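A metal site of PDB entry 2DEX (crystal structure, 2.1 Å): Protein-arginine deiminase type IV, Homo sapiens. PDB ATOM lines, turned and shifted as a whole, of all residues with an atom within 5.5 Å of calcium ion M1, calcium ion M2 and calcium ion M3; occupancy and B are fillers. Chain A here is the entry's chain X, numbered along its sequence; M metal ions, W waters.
NZ of Lys 370 is in salt-bridge range of OD2 of Asp 396, at 3.9 Å. The side-chain carboxylate (OE1) of Glu 260 sits at hydrogen-bond distance from the side-chain amide nitrogen (ND2) of Asn 161 (2.7 Å). N of Cys 174 lies within hydrogen-bond range of O of Asn 161, 3.2 Å away.
Three residues have an atom within 4 Å of calcium ion M3: Asp 173, Asp 176 and Glu 178. The nearest printed residue that does not touch calcium ion M3 is Asp 184 (4.2 Å).
Water W1 bridges OE2 of Glu 260 (2.6 Å) and O of Asp 176 (2.7 Å). Water W2 lies within hydrogen-bond range of the side-chain carboxylate (OE1) of Glu 260 (2.5 Å), the side-chain carboxylate (OD2) of Asp 184 (2.9 Å) and the side-chain amide nitrogen (ND2) of Asn 161 (3.2 Å).
Calcium ion M3 is bound by OD1 of Asp 176 (2.2 Å), water W2 (2.3 Å), O of Glu 178 (2.3 Å), water W1 (2.4 Å) and O of Asp 173 (2.4 Å). Calcium ion M3 has five donor atoms within binding distance.
Of the 22 residues printed, 6 come within 4 Å of calcium ion M2. Along chain A the residues within 4 Å of calcium ion M2 span positions 161 to 187. The nearest printed residue that does not touch calcium ion M2 is Arg 164 (5.0 Å).
Four residues have an atom within 4 Å of calcium ion M1: Asp 163, Asp 165, Asp 187 and Asp 396.
Calcium ion M1 is bound by the side-chain carboxylate (OD1) of Asp 396 (2.3 Å), water W3 (2.4 Å), the side-chain carboxylate (OD2) of Asp 187 (2.4 Å), the side-chain carboxylate (OD2) of Asp 163 (2.5 Å), the side-chain carboxylate (OD2) of Asp 165 (2.6 Å), the side-chain carboxylate (OD1) of Asp 187 (2.7 Å) and the side-chain carboxylate (OD1) of Asp 165 (2.7 Å). Calcium ion M1 has seven donor atoms within binding distance.
Calcium ion M2 is bound by OD1 of Asp 184, OD2 of Asp 187, OD2 of Asp 173, OD1 of Asp 163, OD1 of Asn 161 and OD2 of Asp 165. Calcium ion M2 has six donor atoms within binding distance.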
ATOM      1  N   ASN A 161      -4.661  24.896 -13.255  1.00  0.00           N
ATOM      2  CA  ASN A 161      -4.813  24.929 -14.693  1.00  0.00           C
ATOM      3  C   ASN A 161      -3.472  24.570 -15.343  1.00  0.00           C
ATOM      4  O   ASN A 161      -2.851  25.396 -15.984  1.00  0.00           O
ATOM      5  CB  ASN A 161      -5.341  26.304 -15.155  1.00  0.00           C
ATOM      6  CG  ASN A 161      -5.775  26.311 -16.610  1.00  0.00           C
ATOM      7  OD1 ASN A 161      -5.778  25.267 -17.266  1.00  0.00           O
ATOM      8  ND2 ASN A 161      -6.103  27.496 -17.123  1.00  0.00           N
ATOM      9  N   ASP A 163      -2.552  22.011 -17.591  1.00  0.00           N
ATOM     10  CA  ASP A 163      -2.424  21.409 -18.906  1.00  0.00           C
ATOM     11  C   ASP A 163      -2.055  22.485 -19.922  1.00  0.00           C
ATOM     12  O   ASP A 163      -1.671  23.596 -19.545  1.00  0.00           O
ATOM     13  CB  ASP A 163      -3.694  20.632 -19.297  1.00  0.00           C
ATOM     14  CG  ASP A 163      -4.891  21.526 -19.525  1.00  0.00           C
ATOM     15  OD1 ASP A 163      -4.893  22.687 -19.049  1.00  0.00           O
ATOM     16  OD2 ASP A 163      -5.853  21.058 -20.180  1.00  0.00           O
ATOM     17  N   ARG A 164      -2.132  22.142 -21.197  1.00  0.00           N
ATOM     18  CA  ARG A 164      -1.808  23.101 -22.248  1.00  0.00           C
ATOM     19  C   ARG A 164      -2.786  22.939 -23.389  1.00  0.00           C
ATOM     20  O   ARG A 164      -2.550  22.161 -24.293  1.00  0.00           O
ATOM     21  CB  ARG A 164      -0.377  22.865 -22.742  1.00  0.00           C
ATOM     22  CG  ARG A 164       0.066  23.738 -23.896  1.00  0.00           C
ATOM     23  CD  ARG A 164       1.547  23.555 -24.166  1.00  0.00           C
ATOM     24  NE  ARG A 164       1.863  22.247 -24.765  1.00  0.00           N
ATOM     25  CZ  ARG A 164       2.717  21.349 -24.265  1.00  0.00           C
ATOM     26  NH1 ARG A 164       3.408  21.588 -23.167  1.00  0.00           N
ATOM     27  NH2 ARG A 164       2.907  20.185 -24.889  1.00  0.00           N
ATOM     28  N   ASP A 165      -3.904  23.646 -23.296  1.00  0.00           N
ATOM     29  CA  ASP A 165      -4.858  23.689 -24.394  1.00  0.00           C
ATOM     30  C   ASP A 165      -4.340  24.589 -25.546  1.00  0.00           C
ATOM     31  O   ASP A 165      -4.737  24.400 -26.698  1.00  0.00           O
ATOM     32  CB  ASP A 165      -6.219  24.185 -23.907  1.00  0.00           C
ATOM     33  CG  ASP A 165      -6.834  23.281 -22.876  1.00  0.00           C
ATOM     34  OD1 ASP A 165      -6.952  22.057 -23.119  1.00  0.00           O
ATOM     35  OD2 ASP A 165      -7.206  23.779 -21.801  1.00  0.00           O
ATOM     36  N   ASP A 173      -1.086  26.497 -19.312  1.00  0.00           N
ATOM     37  CA  ASP A 173      -2.038  27.595 -19.554  1.00  0.00           C
ATOM     38  C   ASP A 173      -2.060  28.652 -18.429  1.00  0.00           C
ATOM     39  O   ASP A 173      -2.235  29.828 -18.704  1.00  0.00           O
ATOM     40  CB  ASP A 173      -3.463  27.040 -19.773  1.00  0.00           C
ATOM     41  CG  ASP A 173      -3.607  26.200 -21.040  1.00  0.00           C
ATOM     42  OD1 ASP A 173      -2.927  26.445 -22.075  1.00  0.00           O
ATOM     43  OD2 ASP A 173      -4.464  25.303 -21.000  1.00  0.00           O
ATOM     44  N   CYS A 174      -1.870  28.243 -17.162  1.00  0.00           N
ATOM     45  CA  CYS A 174      -1.953  29.176 -16.018  1.00  0.00           C
ATOM     46  C   CYS A 174      -0.726  30.084 -15.840  1.00  0.00           C
ATOM     47  O   CYS A 174      -0.720  30.939 -14.944  1.00  0.00           O
ATOM     48  CB  CYS A 174      -2.160  28.398 -14.720  1.00  0.00           C
ATOM     49  SG  CYS A 174      -0.766  27.336 -14.382  1.00  0.00           S
ATOM     50  N   GLU A 175       0.317  29.905 -16.661  1.00  0.00           N
ATOM     51  CA  GLU A 175       1.540  30.738 -16.593  1.00  0.00           C
ATOM     52  C   GLU A 175       1.420  32.208 -17.058  1.00  0.00           C
ATOM     53  O   GLU A 175       2.182  33.067 -16.599  1.00  0.00           O
ATOM     54  CB  GLU A 175       2.701  30.070 -17.355  1.00  0.00           C
ATOM     55  CG  GLU A 175       3.303  28.839 -16.628  1.00  0.00           C
ATOM     56  CD  GLU A 175       4.256  28.028 -17.507  1.00  0.00           C
ATOM     57  OE1 GLU A 175       5.057  28.642 -18.263  1.00  0.00           O
ATOM     58  OE2 GLU A 175       4.197  26.772 -17.453  1.00  0.00           O
ATOM     59  N   ASP A 176       0.494  32.515 -17.973  1.00  0.00           N
ATOM     60  CA  ASP A 176       0.263  33.916 -18.410  1.00  0.00           C
ATOM     61  C   ASP A 176      -0.992  34.450 -17.752  1.00  0.00           C
ATOM     62  O   ASP A 176      -1.638  33.739 -16.967  1.00  0.00           O
ATOM     63  CB  ASP A 176       0.119  33.989 -19.937  1.00  0.00           C
ATOM     64  CG  ASP A 176      -1.099  33.221 -20.460  1.00  0.00           C
ATOM     65  OD1 ASP A 176      -1.896  32.714 -19.609  1.00  0.00           O
ATOM     66  OD2 ASP A 176      -1.260  33.096 -21.693  1.00  0.00           O
ATOM     67  N   ASP A 177      -1.355  35.685 -18.064  1.00  0.00           N
ATOM     68  CA  ASP A 177      -2.609  36.291 -17.544  1.00  0.00           C
ATOM     69  C   ASP A 177      -3.613  36.568 -18.663  1.00  0.00           C
ATOM     70  O   ASP A 177      -4.192  37.660 -18.747  1.00  0.00           O
ATOM     71  CB  ASP A 177      -2.348  37.546 -16.702  1.00  0.00           C
ATOM     72  CG  ASP A 177      -1.062  38.242 -17.063  1.00  0.00           C
ATOM     73  OD1 ASP A 177      -1.038  39.037 -18.048  1.00  0.00           O
ATOM     74  OD2 ASP A 177      -0.060  37.959 -16.363  1.00  0.00           O
ATOM     75  N   GLU A 178      -3.801  35.561 -19.518  1.00  0.00           N
ATOM     76  CA  GLU A 178      -4.811  35.619 -20.563  1.00  0.00           C
ATOM     77  C   GLU A 178      -5.506  34.287 -20.708  1.00  0.00           C
ATOM     78  O   GLU A 178      -4.901  33.247 -20.474  1.00  0.00           O
ATOM     79  CB  GLU A 178      -4.163  35.965 -21.891  1.00  0.00           C
ATOM     80  CG  GLU A 178      -3.326  37.206 -21.830  1.00  0.00           C
ATOM     81  CD  GLU A 178      -2.952  37.727 -23.195  1.00  0.00           C
ATOM     82  OE1 GLU A 178      -3.832  37.725 -24.074  1.00  0.00           O
ATOM     83  OE2 GLU A 178      -1.789  38.131 -23.371  1.00  0.00           O
ATOM     84  N   VAL A 179      -6.774  34.307 -21.087  1.00  0.00           N
ATOM     85  CA  VAL A 179      -7.447  33.103 -21.562  1.00  0.00           C
ATOM     86  C   VAL A 179      -7.258  33.122 -23.080  1.00  0.00           C
ATOM     87  O   VAL A 179      -7.775  34.013 -23.755  1.00  0.00           O
ATOM     88  CB  VAL A 179      -8.948  33.094 -21.216  1.00  0.00           C
ATOM     89  CG1 VAL A 179      -9.584  31.766 -21.606  1.00  0.00           C
ATOM     90  CG2 VAL A 179      -9.144  33.345 -19.747  1.00  0.00           C
ATOM     91  N   LEU A 180      -6.480  32.174 -23.596  1.00  0.00           N
ATOM     92  CA  LEU A 180      -6.086  32.192 -25.008  1.00  0.00           C
ATOM     93  C   LEU A 180      -6.932  31.273 -25.884  1.00  0.00           C
ATOM     94  O   LEU A 180      -6.851  31.357 -27.109  1.00  0.00           O
ATOM     95  CB  LEU A 180      -4.605  31.818 -25.162  1.00  0.00           C
ATOM     96  CG  LEU A 180      -3.633  32.917 -24.725  1.00  0.00           C
ATOM     97  CD1 LEU A 180      -2.218  32.402 -24.863  1.00  0.00           C
ATOM     98  CD2 LEU A 180      -3.830  34.205 -25.527  1.00  0.00           C
ATOM     99  N   GLU A 183     -11.743  26.758 -24.941  1.00  0.00           N
ATOM    100  CA  GLU A 183     -11.785  25.478 -24.229  1.00  0.00           C
ATOM    101  C   GLU A 183     -10.972  25.473 -22.930  1.00  0.00           C
ATOM    102  O   GLU A 183     -11.201  24.633 -22.076  1.00  0.00           O
ATOM    103  CB  GLU A 183     -11.364  24.289 -25.130  1.00  0.00           C
ATOM    104  CG  GLU A 183     -10.264  24.567 -26.187  1.00  0.00           C
ATOM    105  CD  GLU A 183     -10.774  25.289 -27.433  1.00  0.00           C
ATOM    106  OE1 GLU A 183     -11.944  25.079 -27.839  1.00  0.00           O
ATOM    107  OE2 GLU A 183      -9.992  26.073 -28.003  1.00  0.00           O
ATOM    108  N   ASP A 184     -10.035  26.392 -22.796  1.00  0.00           N
ATOM    109  CA  ASP A 184      -9.308  26.588 -21.550  1.00  0.00           C
ATOM    110  C   ASP A 184     -10.305  26.870 -20.414  1.00  0.00           C
ATOM    111  O   ASP A 184     -10.141  26.348 -19.290  1.00  0.00           O
ATOM    112  CB  ASP A 184      -8.312  27.743 -21.682  1.00  0.00           C
ATOM    113  CG  ASP A 184      -7.382  27.864 -20.485  1.00  0.00           C
ATOM    114  OD1 ASP A 184      -6.960  26.801 -19.953  1.00  0.00           O
ATOM    115  OD2 ASP A 184      -7.068  29.005 -20.093  1.00  0.00           O
ATOM    116  N   ASP A 187     -11.649  24.286 -18.004  1.00  0.00           N
ATOM    117  CA  ASP A 187     -10.838  23.863 -16.878  1.00  0.00           C
ATOM    118  C   ASP A 187     -11.090  24.746 -15.678  1.00  0.00           C
ATOM    119  O   ASP A 187     -10.793  24.338 -14.564  1.00  0.00           O
ATOM    120  CB  ASP A 187      -9.348  23.933 -17.205  1.00  0.00           C
ATOM    121  CG  ASP A 187      -8.945  22.987 -18.298  1.00  0.00           C
ATOM    122  OD1 ASP A 187      -9.569  21.911 -18.426  1.00  0.00           O
ATOM    123  OD2 ASP A 187      -8.008  23.336 -19.041  1.00  0.00           O
ATOM    124  N   MET A 188     -11.606  25.948 -15.911  1.00  0.00           N
ATOM    125  CA  MET A 188     -11.753  26.959 -14.858  1.00  0.00           C
ATOM    126  C   MET A 188     -13.081  26.862 -14.126  1.00  0.00           C
ATOM    127  O   MET A 188     -14.029  26.290 -14.620  1.00  0.00           O
ATOM    128  CB  MET A 188     -11.592  28.338 -15.477  1.00  0.00           C
ATOM    129  CG  MET A 188     -10.248  28.518 -16.139  1.00  0.00           C
ATOM    130  SD  MET A 188      -9.992  30.212 -16.685  1.00  0.00           S
ATOM    131  CE  MET A 188      -8.579  30.027 -17.712  1.00  0.00           C
ATOM    132  N   PHE A 222     -10.604  35.821 -13.954  1.00  0.00           N
ATOM    133  CA  PHE A 222     -10.950  36.544 -15.197  1.00  0.00           C
ATOM    134  C   PHE A 222     -12.411  36.950 -15.188  1.00  0.00           C
ATOM    135  O   PHE A 222     -13.274  36.195 -14.748  1.00  0.00           O
ATOM    136  CB  PHE A 222     -10.742  35.656 -16.439  1.00  0.00           C
ATOM    137  CG  PHE A 222      -9.317  35.255 -16.681  1.00  0.00           C
ATOM    138  CD1 PHE A 222      -8.811  34.088 -16.143  1.00  0.00           C
ATOM    139  CD2 PHE A 222      -8.486  36.054 -17.477  1.00  0.00           C
ATOM    140  CE1 PHE A 222      -7.499  33.716 -16.357  1.00  0.00           C
ATOM    141  CE2 PHE A 222      -7.161  35.686 -17.708  1.00  0.00           C
ATOM    142  CZ  PHE A 222      -6.672  34.520 -17.131  1.00  0.00           C
ATOM    143  N   GLU A 260      -8.930  30.165 -12.109  1.00  0.00           N
ATOM    144  CA  GLU A 260      -7.949  29.072 -12.288  1.00  0.00           C
ATOM    145  C   GLU A 260      -7.049  29.077 -11.074  1.00  0.00           C
ATOM    146  O   GLU A 260      -6.735  30.151 -10.535  1.00  0.00           O
ATOM    147  CB  GLU A 260      -7.151  29.235 -13.611  1.00  0.00           C
ATOM    148  CG  GLU A 260      -6.356  30.534 -13.717  1.00  0.00           C
ATOM    149  CD  GLU A 260      -5.532  30.683 -14.982  1.00  0.00           C
ATOM    150  OE1 GLU A 260      -5.563  29.818 -15.890  1.00  0.00           O
ATOM    151  OE2 GLU A 260      -4.835  31.701 -15.086  1.00  0.00           O
ATOM    152  N   LYS A 370     -14.960  19.133 -14.468  1.00  0.00           N
ATOM    153  CA  LYS A 370     -13.857  18.691 -15.302  1.00  0.00           C
ATOM    154  C   LYS A 370     -12.916  17.745 -14.538  1.00  0.00           C
ATOM    155  O   LYS A 370     -12.623  17.955 -13.369  1.00  0.00           O
ATOM    156  CB  LYS A 370     -13.084  19.920 -15.835  1.00  0.00           C
ATOM    157  CG  LYS A 370     -11.791  19.586 -16.623  1.00  0.00           C
ATOM    158  CD  LYS A 370     -12.098  18.936 -18.008  1.00  0.00           C
ATOM    159  CE  LYS A 370     -12.002  19.953 -19.131  1.00  0.00           C
ATOM    160  NZ  LYS A 370     -12.724  19.561 -20.375  1.00  0.00           N
ATOM    161  N   LEU A 372      -9.178  15.705 -15.459  1.00  0.00           N
ATOM    162  CA  LEU A 372      -8.146  15.471 -16.479  1.00  0.00           C
ATOM    163  C   LEU A 372      -6.948  14.728 -15.925  1.00  0.00           C
ATOM    164  O   LEU A 372      -6.644  14.836 -14.744  1.00  0.00           O
ATOM    165  CB  LEU A 372      -7.671  16.771 -17.129  1.00  0.00           C
ATOM    166  CG  LEU A 372      -7.109  17.901 -16.270  1.00  0.00           C
ATOM    167  CD1 LEU A 372      -5.975  18.662 -16.977  1.00  0.00           C
ATOM    168  CD2 LEU A 372      -8.203  18.853 -15.925  1.00  0.00           C
ATOM    169  N   PRO A 395      -3.079  19.269 -24.579  1.00  0.00           N
ATOM    170  CA  PRO A 395      -4.499  19.531 -24.352  1.00  0.00           C
ATOM    171  C   PRO A 395      -5.159  18.469 -23.450  1.00  0.00           C
ATOM    172  O   PRO A 395      -5.089  17.283 -23.748  1.00  0.00           O
ATOM    173  CB  PRO A 395      -5.099  19.508 -25.772  1.00  0.00           C
ATOM    174  CG  PRO A 395      -3.939  19.905 -26.663  1.00  0.00           C
ATOM    175  CD  PRO A 395      -2.763  19.174 -26.018  1.00  0.00           C
ATOM    176  N   ASP A 396      -5.759  18.927 -22.353  1.00  0.00           N
ATOM    177  CA  ASP A 396      -6.377  18.043 -21.331  1.00  0.00           C
ATOM    178  C   ASP A 396      -5.438  16.981 -20.739  1.00  0.00           C
ATOM    179  O   ASP A 396      -5.857  15.935 -20.249  1.00  0.00           O
ATOM    180  CB  ASP A 396      -7.707  17.455 -21.833  1.00  0.00           C
ATOM    181  CG  ASP A 396      -8.849  18.480 -21.796  1.00  0.00           C
ATOM    182  OD1 ASP A 396      -8.794  19.422 -20.978  1.00  0.00           O
ATOM    183  OD2 ASP A 396      -9.781  18.355 -22.591  1.00  0.00           O
HETATM  184 CA    CA M   1      -8.228  21.657 -20.748  1.00  0.00          CA
HETATM  185 CA    CA M   2      -6.224  24.655 -19.650  1.00  0.00          CA
HETATM  186 CA    CA M   3      -3.746  31.472 -19.625  1.00  0.00          CA
HETATM  187  O   HOH W   1      -3.833  32.310 -17.385  1.00  0.00           O
HETATM  188  O   HOH W   2      -5.191  30.278 -18.354  1.00  0.00           O
HETATM  189  O   HOH W   3     -10.126  22.415 -21.916  1.00  0.00           O
